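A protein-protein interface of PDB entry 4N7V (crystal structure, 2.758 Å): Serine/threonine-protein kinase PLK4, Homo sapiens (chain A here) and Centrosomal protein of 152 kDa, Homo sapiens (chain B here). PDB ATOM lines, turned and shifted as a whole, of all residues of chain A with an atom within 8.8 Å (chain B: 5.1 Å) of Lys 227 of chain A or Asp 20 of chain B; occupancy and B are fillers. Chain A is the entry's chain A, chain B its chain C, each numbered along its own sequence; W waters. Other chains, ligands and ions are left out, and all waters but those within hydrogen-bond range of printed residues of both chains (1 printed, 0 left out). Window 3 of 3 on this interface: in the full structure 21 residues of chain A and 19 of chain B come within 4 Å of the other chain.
The side-chain amino group of Lys 132 of chain A lies within salt-bridge range of the side-chain carboxylate of Asp 23 of chain B, 3.6 Å away. The side-chain amino group (NZ) of Lys 132 of chain A lies within salt-bridge range of the side-chain carboxylate (OD1) of Asp 20 of chain B (3.3 Å). NZ of Lys 132 of chain A lies within salt-bridge range of OE2 of Glu 22 of chain B, at 3.7 Å. The side-chain amino group (NZ) of Lys 227 of chain A is in salt-bridge range of the side-chain carboxylate (OD1) of Asp 20 of chain B (3.2 Å).
The backbone NH (N) of Lys 132 of chain A sits at hydrogen-bond distance from the backbone carbonyl oxygen (O) of Trp 147 of chain A, at 2.9 Å. The side-chain carboxylate (OD2) of Asp 20 of chain B lies close to the backbone NH (N) of Glu 22 of chain B. OD2 of Asp 20 of chain B sits at hydrogen-bond distance from N of Asp 23 of chain B (3.1 Å).
Glu 22 of chain B touches Ile 134 of chain A. Trp 147 of chain A touches Glu 21 of chain B (CZ3 to CG, 3.5 Å). CG of Glu 22 of chain B touches CD2 of Trp 147 of chain A (3.5 Å).
Lys 227 of chain A touches one residue of chain B. Of chain A, only Lys 132 (3.3 Å) and Lys 227 (3.2 Å) come within 4 Å of Asp 20 of chain B. Printed residues of chain B within 4 Å of Trp 147 of chain A: Glu 21 and Glu 22. Of the printed residues of chain B, Lys 132 of chain A touches Asp 20 (3.3 Å), Glu 22 (3.4 Å) and Asp 23 (3.6 Å). Of the printed residues of chain B, Ile 134 of chain A touches Glu 22 (3.2 Å). The nearest printed residue of chain B that does not touch Lys 132 of chain A is Glu 21 of chain B (6.4 Å).
Of the 8 printed residues of chain B, 4 touch a printed residue of chain A. Among the printed residues, Asp or Glu carboxylates within 4 Å of a Lys or Arg side-chain nitrogen of the other chain: Lys 132 of chain A with Asp 20 of chain B (3.3 Å), Lys 132 of chain A with Glu 22 of chain B (3.7 Å), Lys 132 of chain A with Asp 23 of chain B (3.6 Å) and Lys 227 of chain A with Asp 20 of chain B (3.2 Å).
Water W1 lies within hydrogen-bond range of the side-chain carboxylate of Asp 23 of chain B and the side-chain amino group of Lys 132 of chain A.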
ATOM      1  N   THR A 125      32.698  12.286  16.006  1.00  0.00           N
ATOM      2  CA  THR A 125      31.961  11.848  17.180  1.00  0.00           C
ATOM      3  C   THR A 125      32.689  10.681  17.827  1.00  0.00           C
ATOM      4  O   THR A 125      32.901   9.647  17.192  1.00  0.00           O
ATOM      5  CB  THR A 125      30.523  11.438  16.829  1.00  0.00           C
ATOM      6  OG1 THR A 125      29.793  12.595  16.406  1.00  0.00           O
ATOM      7  CG2 THR A 125      29.833  10.824  18.034  1.00  0.00           C
ATOM      8  N   TYR A 126      33.081  10.858  19.086  1.00  0.00           N
ATOM      9  CA  TYR A 126      33.851   9.847  19.809  1.00  0.00           C
ATOM     10  C   TYR A 126      33.145   9.396  21.086  1.00  0.00           C
ATOM     11  O   TYR A 126      32.760  10.217  21.921  1.00  0.00           O
ATOM     12  CB  TYR A 126      35.254  10.373  20.129  1.00  0.00           C
ATOM     13  CG  TYR A 126      36.159   9.374  20.818  1.00  0.00           C
ATOM     14  CD1 TYR A 126      36.286   8.078  20.342  1.00  0.00           C
ATOM     15  CD2 TYR A 126      36.902   9.739  21.935  1.00  0.00           C
ATOM     16  CE1 TYR A 126      37.120   7.167  20.971  1.00  0.00           C
ATOM     17  CE2 TYR A 126      37.736   8.840  22.566  1.00  0.00           C
ATOM     18  CZ  TYR A 126      37.842   7.558  22.083  1.00  0.00           C
ATOM     19  OH  TYR A 126      38.676   6.669  22.720  1.00  0.00           O
ATOM     20  N   PHE A 127      32.977   8.086  21.226  1.00  0.00           N
ATOM     21  CA  PHE A 127      32.316   7.521  22.395  1.00  0.00           C
ATOM     22  C   PHE A 127      33.320   6.931  23.372  1.00  0.00           C
ATOM     23  O   PHE A 127      33.950   5.912  23.087  1.00  0.00           O
ATOM     24  CB  PHE A 127      31.313   6.448  21.976  1.00  0.00           C
ATOM     25  CG  PHE A 127      30.061   7.000  21.372  1.00  0.00           C
ATOM     26  CD1 PHE A 127      29.059   7.505  22.180  1.00  0.00           C
ATOM     27  CD2 PHE A 127      29.886   7.016  20.000  1.00  0.00           C
ATOM     28  CE1 PHE A 127      27.903   8.017  21.633  1.00  0.00           C
ATOM     29  CE2 PHE A 127      28.729   7.528  19.444  1.00  0.00           C
ATOM     30  CZ  PHE A 127      27.735   8.029  20.263  1.00  0.00           C
ATOM     31  N   THR A 128      33.469   7.581  24.522  1.00  0.00           N
ATOM     32  CA  THR A 128      34.325   7.067  25.582  1.00  0.00           C
ATOM     33  C   THR A 128      33.524   6.171  26.517  1.00  0.00           C
ATOM     34  O   THR A 128      32.347   5.894  26.267  1.00  0.00           O
ATOM     35  CB  THR A 128      34.954   8.204  26.405  1.00  0.00           C
ATOM     36  OG1 THR A 128      33.930   8.906  27.121  1.00  0.00           O
ATOM     37  CG2 THR A 128      35.695   9.177  25.503  1.00  0.00           C
ATOM     38  N   ARG A 129      34.168   5.719  27.589  1.00  0.00           N
ATOM     39  CA  ARG A 129      33.499   4.909  28.602  1.00  0.00           C
ATOM     40  C   ARG A 129      32.500   5.746  29.398  1.00  0.00           C
ATOM     41  O   ARG A 129      31.483   5.235  29.875  1.00  0.00           O
ATOM     42  CB  ARG A 129      34.530   4.256  29.531  1.00  0.00           C
ATOM     43  CG  ARG A 129      34.058   4.032  30.968  1.00  0.00           C
ATOM     44  CD  ARG A 129      34.366   2.627  31.468  1.00  0.00           C
ATOM     45  NE  ARG A 129      34.163   2.506  32.912  1.00  0.00           N
ATOM     46  CZ  ARG A 129      32.997   2.227  33.489  1.00  0.00           C
ATOM     47  NH1 ARG A 129      31.913   2.040  32.749  1.00  0.00           N
ATOM     48  NH2 ARG A 129      32.915   2.138  34.811  1.00  0.00           N
ATOM     49  N   ALA A 131      31.524   9.243  28.362  1.00  0.00           N
ATOM     50  CA  ALA A 131      30.915  10.369  27.657  1.00  0.00           C
ATOM     51  C   ALA A 131      30.831  10.222  26.141  1.00  0.00           C
ATOM     52  O   ALA A 131      31.469   9.351  25.547  1.00  0.00           O
ATOM     53  CB  ALA A 131      31.647  11.656  28.007  1.00  0.00           C
ATOM     54  N   LYS A 132      30.028  11.092  25.534  1.00  0.00           N
ATOM     55  CA  LYS A 132      29.959  11.235  24.083  1.00  0.00           C
ATOM     56  C   LYS A 132      30.676  12.523  23.692  1.00  0.00           C
ATOM     57  O   LYS A 132      30.281  13.612  24.110  1.00  0.00           O
ATOM     58  CB  LYS A 132      28.500  11.289  23.612  1.00  0.00           C
ATOM     59  CG  LYS A 132      28.325  11.520  22.116  1.00  0.00           C
ATOM     60  CD  LYS A 132      26.886  11.854  21.766  1.00  0.00           C
ATOM     61  CE  LYS A 132      26.721  12.071  20.267  1.00  0.00           C
ATOM     62  NZ  LYS A 132      25.366  12.595  19.915  1.00  0.00           N
ATOM     63  N   ILE A 134      32.154  15.261  20.837  1.00  0.00           N
ATOM     64  CA  ILE A 134      31.902  15.782  19.498  1.00  0.00           C
ATOM     65  C   ILE A 134      32.774  16.991  19.160  1.00  0.00           C
ATOM     66  O   ILE A 134      32.650  18.055  19.767  1.00  0.00           O
ATOM     67  CB  ILE A 134      30.430  16.192  19.318  1.00  0.00           C
ATOM     68  CG1 ILE A 134      29.503  15.006  19.584  1.00  0.00           C
ATOM     69  CG2 ILE A 134      30.198  16.734  17.918  1.00  0.00           C
ATOM     70  CD1 ILE A 134      28.053  15.309  19.322  1.00  0.00           C
ATOM     71  N   TRP A 147      29.020  15.328  26.218  1.00  0.00           N
ATOM     72  CA  TRP A 147      27.848  14.902  26.966  1.00  0.00           C
ATOM     73  C   TRP A 147      28.124  13.600  27.702  1.00  0.00           C
ATOM     74  O   TRP A 147      28.049  12.520  27.115  1.00  0.00           O
ATOM     75  CB  TRP A 147      26.645  14.729  26.040  1.00  0.00           C
ATOM     76  CG  TRP A 147      25.845  15.974  25.861  1.00  0.00           C
ATOM     77  CD1 TRP A 147      26.322  17.241  25.684  1.00  0.00           C
ATOM     78  CD2 TRP A 147      24.417  16.078  25.866  1.00  0.00           C
ATOM     79  NE1 TRP A 147      25.277  18.126  25.567  1.00  0.00           N
ATOM     80  CE2 TRP A 147      24.097  17.436  25.676  1.00  0.00           C
ATOM     81  CE3 TRP A 147      23.379  15.151  26.006  1.00  0.00           C
ATOM     82  CZ2 TRP A 147      22.781  17.892  25.625  1.00  0.00           C
ATOM     83  CZ3 TRP A 147      22.073  15.606  25.956  1.00  0.00           C
ATOM     84  CH2 TRP A 147      21.785  16.964  25.766  1.00  0.00           C
ATOM     85  N   TYR A 149      27.453  10.451  29.994  1.00  0.00           N
ATOM     86  CA  TYR A 149      26.292   9.612  30.261  1.00  0.00           C
ATOM     87  C   TYR A 149      25.857   9.877  31.697  1.00  0.00           C
ATOM     88  O   TYR A 149      24.689   9.715  32.052  1.00  0.00           O
ATOM     89  CB  TYR A 149      26.650   8.136  30.092  1.00  0.00           C
ATOM     90  CG  TYR A 149      27.467   7.827  28.858  1.00  0.00           C
ATOM     91  CD1 TYR A 149      27.182   8.426  27.638  1.00  0.00           C
ATOM     92  CD2 TYR A 149      28.529   6.934  28.914  1.00  0.00           C
ATOM     93  CE1 TYR A 149      27.927   8.145  26.509  1.00  0.00           C
ATOM     94  CE2 TYR A 149      29.280   6.646  27.792  1.00  0.00           C
ATOM     95  CZ  TYR A 149      28.975   7.254  26.591  1.00  0.00           C
ATOM     96  OH  TYR A 149      29.720   6.971  25.466  1.00  0.00           O
ATOM     97  N   ILE A 223      31.915   8.777  12.975  1.00  0.00           N
ATOM     98  CA  ILE A 223      31.376   8.324  14.248  1.00  0.00           C
ATOM     99  C   ILE A 223      32.213   7.161  14.760  1.00  0.00           C
ATOM    100  O   ILE A 223      32.215   6.077  14.178  1.00  0.00           O
ATOM    101  CB  ILE A 223      29.907   7.902  14.124  1.00  0.00           C
ATOM    102  CG1 ILE A 223      29.060   9.092  13.671  1.00  0.00           C
ATOM    103  CG2 ILE A 223      29.406   7.366  15.452  1.00  0.00           C
ATOM    104  CD1 ILE A 223      27.607   8.760  13.434  1.00  0.00           C
ATOM    105  N   ILE A 224      32.931   7.398  15.850  1.00  0.00           N
ATOM    106  CA  ILE A 224      33.854   6.404  16.374  1.00  0.00           C
ATOM    107  C   ILE A 224      33.350   5.747  17.656  1.00  0.00           C
ATOM    108  O   ILE A 224      32.991   6.427  18.620  1.00  0.00           O
ATOM    109  CB  ILE A 224      35.237   7.018  16.620  1.00  0.00           C
ATOM    110  CG1 ILE A 224      35.732   7.707  15.346  1.00  0.00           C
ATOM    111  CG2 ILE A 224      36.213   5.953  17.076  1.00  0.00           C
ATOM    112  CD1 ILE A 224      37.158   8.203  15.426  1.00  0.00           C
ATOM    113  N   GLY A 225      33.332   4.418  17.658  1.00  0.00           N
ATOM    114  CA  GLY A 225      32.856   3.670  18.806  1.00  0.00           C
ATOM    115  C   GLY A 225      31.344   3.681  18.858  1.00  0.00           C
ATOM    116  O   GLY A 225      30.689   4.144  17.924  1.00  0.00           O
ATOM    117  N   ARG A 226      30.782   3.169  19.947  1.00  0.00           N
ATOM    118  CA  ARG A 226      29.334   3.128  20.105  1.00  0.00           C
ATOM    119  C   ARG A 226      28.926   3.407  21.543  1.00  0.00           C
ATOM    120  O   ARG A 226      29.626   3.028  22.482  1.00  0.00           O
ATOM    121  CB  ARG A 226      28.771   1.779  19.645  1.00  0.00           C
ATOM    122  CG  ARG A 226      29.311   0.574  20.400  1.00  0.00           C
ATOM    123  CD  ARG A 226      28.580  -0.696  19.990  1.00  0.00           C
ATOM    124  NE  ARG A 226      28.971  -1.171  18.665  1.00  0.00           N
ATOM    125  CZ  ARG A 226      29.871  -2.126  18.457  1.00  0.00           C
ATOM    126  NH1 ARG A 226      30.471  -2.703  19.490  1.00  0.00           N
ATOM    127  NH2 ARG A 226      30.171  -2.506  17.223  1.00  0.00           N
ATOM    128  N   LYS A 227      27.794   4.086  21.703  1.00  0.00           N
ATOM    129  CA  LYS A 227      27.242   4.383  23.018  1.00  0.00           C
ATOM    130  C   LYS A 227      26.904   3.099  23.771  1.00  0.00           C
ATOM    131  O   LYS A 227      26.058   2.319  23.341  1.00  0.00           O
ATOM    132  CB  LYS A 227      26.009   5.284  22.879  1.00  0.00           C
ATOM    133  CG  LYS A 227      25.188   5.009  21.619  1.00  0.00           C
ATOM    134  CD  LYS A 227      24.432   6.245  21.108  1.00  0.00           C
ATOM    135  CE  LYS A 227      23.397   6.761  22.108  1.00  0.00           C
ATOM    136  NZ  LYS A 227      23.817   8.043  22.761  1.00  0.00           N
ATOM    137  N   PRO A 228      27.570   2.882  24.911  1.00  0.00           N
ATOM    138  CA  PRO A 228      27.447   1.628  25.656  1.00  0.00           C
ATOM    139  C   PRO A 228      26.242   1.621  26.596  1.00  0.00           C
ATOM    140  O   PRO A 228      25.459   0.672  26.571  1.00  0.00           O
ATOM    141  CB  PRO A 228      28.758   1.573  26.447  1.00  0.00           C
ATOM    142  CG  PRO A 228      29.225   3.018  26.555  1.00  0.00           C
ATOM    143  CD  PRO A 228      28.402   3.867  25.620  1.00  0.00           C
ATOM    144  N   GLU B  17      21.899   4.086  14.839  1.00  0.00           N
ATOM    145  CA  GLU B  17      20.809   4.802  15.494  1.00  0.00           C
ATOM    146  C   GLU B  17      20.592   6.182  14.886  1.00  0.00           C
ATOM    147  O   GLU B  17      21.366   6.631  14.040  1.00  0.00           O
ATOM    148  CB  GLU B  17      21.062   4.923  17.001  1.00  0.00           C
ATOM    149  CG  GLU B  17      20.901   3.618  17.771  1.00  0.00           C
ATOM    150  CD  GLU B  17      22.054   2.658  17.550  1.00  0.00           C
ATOM    151  OE1 GLU B  17      21.808   1.434  17.502  1.00  0.00           O
ATOM    152  OE2 GLU B  17      23.207   3.126  17.432  1.00  0.00           O
ATOM    153  N   GLU B  18      19.532   6.854  15.323  1.00  0.00           N
ATOM    154  CA  GLU B  18      19.214   8.176  14.809  1.00  0.00           C
ATOM    155  C   GLU B  18      19.544   9.268  15.821  1.00  0.00           C
ATOM    156  O   GLU B  18      20.473   9.139  16.620  1.00  0.00           O
ATOM    157  CB  GLU B  18      17.733   8.266  14.425  1.00  0.00           C
ATOM    158  CG  GLU B  18      17.250   7.181  13.471  1.00  0.00           C
ATOM    159  CD  GLU B  18      16.789   5.922  14.189  1.00  0.00           C
ATOM    160  OE1 GLU B  18      17.345   5.599  15.261  1.00  0.00           O
ATOM    161  OE2 GLU B  18      15.861   5.258  13.680  1.00  0.00           O
ATOM    162  N   TYR B  19      18.764  10.341  15.772  1.00  0.00           N
ATOM    163  CA  TYR B  19      18.930  11.479  16.666  1.00  0.00           C
ATOM    164  C   TYR B  19      18.688  11.098  18.125  1.00  0.00           C
ATOM    165  O   TYR B  19      17.634  10.558  18.465  1.00  0.00           O
ATOM    166  CB  TYR B  19      17.962  12.593  16.260  1.00  0.00           C
ATOM    167  CG  TYR B  19      18.561  13.699  15.410  1.00  0.00           C
ATOM    168  CD1 TYR B  19      18.274  15.034  15.678  1.00  0.00           C
ATOM    169  CD2 TYR B  19      19.409  13.415  14.345  1.00  0.00           C
ATOM    170  CE1 TYR B  19      18.810  16.053  14.913  1.00  0.00           C
ATOM    171  CE2 TYR B  19      19.952  14.434  13.572  1.00  0.00           C
ATOM    172  CZ  TYR B  19      19.646  15.751  13.864  1.00  0.00           C
ATOM    173  OH  TYR B  19      20.172  16.774  13.110  1.00  0.00           O
ATOM    174  N   ASP B  20      19.667  11.372  18.983  1.00  0.00           N
ATOM    175  CA  ASP B  20      19.455  11.277  20.426  1.00  0.00           C
ATOM    176  C   ASP B  20      19.184  12.665  21.013  1.00  0.00           C
ATOM    177  O   ASP B  20      18.882  13.602  20.275  1.00  0.00           O
ATOM    178  CB  ASP B  20      20.642  10.603  21.120  1.00  0.00           C
ATOM    179  CG  ASP B  20      21.972  11.264  20.793  1.00  0.00           C
ATOM    180  OD1 ASP B  20      23.019  10.688  21.155  1.00  0.00           O
ATOM    181  OD2 ASP B  20      21.978  12.351  20.178  1.00  0.00           O
ATOM    182  N   GLU B  21      19.286  12.799  22.332  1.00  0.00           N
ATOM    183  CA  GLU B  21      19.057  14.094  22.970  1.00  0.00           C
ATOM    184  C   GLU B  21      20.116  15.115  22.564  1.00  0.00           C
ATOM    185  O   GLU B  21      19.809  16.289  22.359  1.00  0.00           O
ATOM    186  CB  GLU B  21      19.017  13.968  24.495  1.00  0.00           C
ATOM    187  CG  GLU B  21      18.641  15.269  25.206  1.00  0.00           C
ATOM    188  CD  GLU B  21      18.374  15.078  26.688  1.00  0.00           C
ATOM    189  OE1 GLU B  21      18.663  13.981  27.212  1.00  0.00           O
ATOM    190  OE2 GLU B  21      17.871  16.024  27.329  1.00  0.00           O
ATOM    191  N   GLU B  22      21.360  14.657  22.457  1.00  0.00           N
ATOM    192  CA  GLU B  22      22.481  15.526  22.120  1.00  0.00           C
ATOM    193  C   GLU B  22      22.252  16.163  20.756  1.00  0.00           C
ATOM    194  O   GLU B  22      22.572  17.333  20.538  1.00  0.00           O
ATOM    195  CB  GLU B  22      23.779  14.719  22.114  1.00  0.00           C
ATOM    196  CG  GLU B  22      25.020  15.500  22.517  1.00  0.00           C
ATOM    197  CD  GLU B  22      25.481  16.485  21.458  1.00  0.00           C
ATOM    198  OE1 GLU B  22      26.149  17.476  21.825  1.00  0.00           O
ATOM    199  OE2 GLU B  22      25.187  16.270  20.264  1.00  0.00           O
ATOM    200  N   ASP B  23      21.687  15.382  19.844  1.00  0.00           N
ATOM    201  CA  ASP B  23      21.421  15.848  18.491  1.00  0.00           C
ATOM    202  C   ASP B  23      20.304  16.892  18.439  1.00  0.00           C
ATOM    203  O   ASP B  23      20.473  17.954  17.842  1.00  0.00           O
ATOM    204  CB  ASP B  23      21.090  14.669  17.577  1.00  0.00           C
ATOM    205  CG  ASP B  23      22.269  13.740  17.376  1.00  0.00           C
ATOM    206  OD1 ASP B  23      23.413  14.233  17.303  1.00  0.00           O
ATOM    207  OD2 ASP B  23      22.051  12.515  17.284  1.00  0.00           O
ATOM    208  N   TYR B  24      19.171  16.589  19.066  1.00  0.00           N
ATOM    209  CA  TYR B  24      18.026  17.497  19.062  1.00  0.00           C
ATOM    210  C   TYR B  24      18.328  18.812  19.774  1.00  0.00           C
ATOM    211  O   TYR B  24      17.849  19.870  19.368  1.00  0.00           O
ATOM    212  CB  TYR B  24      16.804  16.831  19.700  1.00  0.00           C
ATOM    213  CG  TYR B  24      16.167  15.757  18.848  1.00  0.00           C
ATOM    214  CD1 TYR B  24      16.091  14.444  19.294  1.00  0.00           C
ATOM    215  CD2 TYR B  24      15.642  16.054  17.599  1.00  0.00           C
ATOM    216  CE1 TYR B  24      15.505  13.458  18.527  1.00  0.00           C
ATOM    217  CE2 TYR B  24      15.061  15.070  16.821  1.00  0.00           C
ATOM    218  CZ  TYR B  24      14.993  13.775  17.292  1.00  0.00           C
ATOM    219  OH  TYR B  24      14.412  12.796  16.521  1.00  0.00           O
HETATM  220  O   HOH W   1      24.507  11.099  17.564  1.00  0.00           O
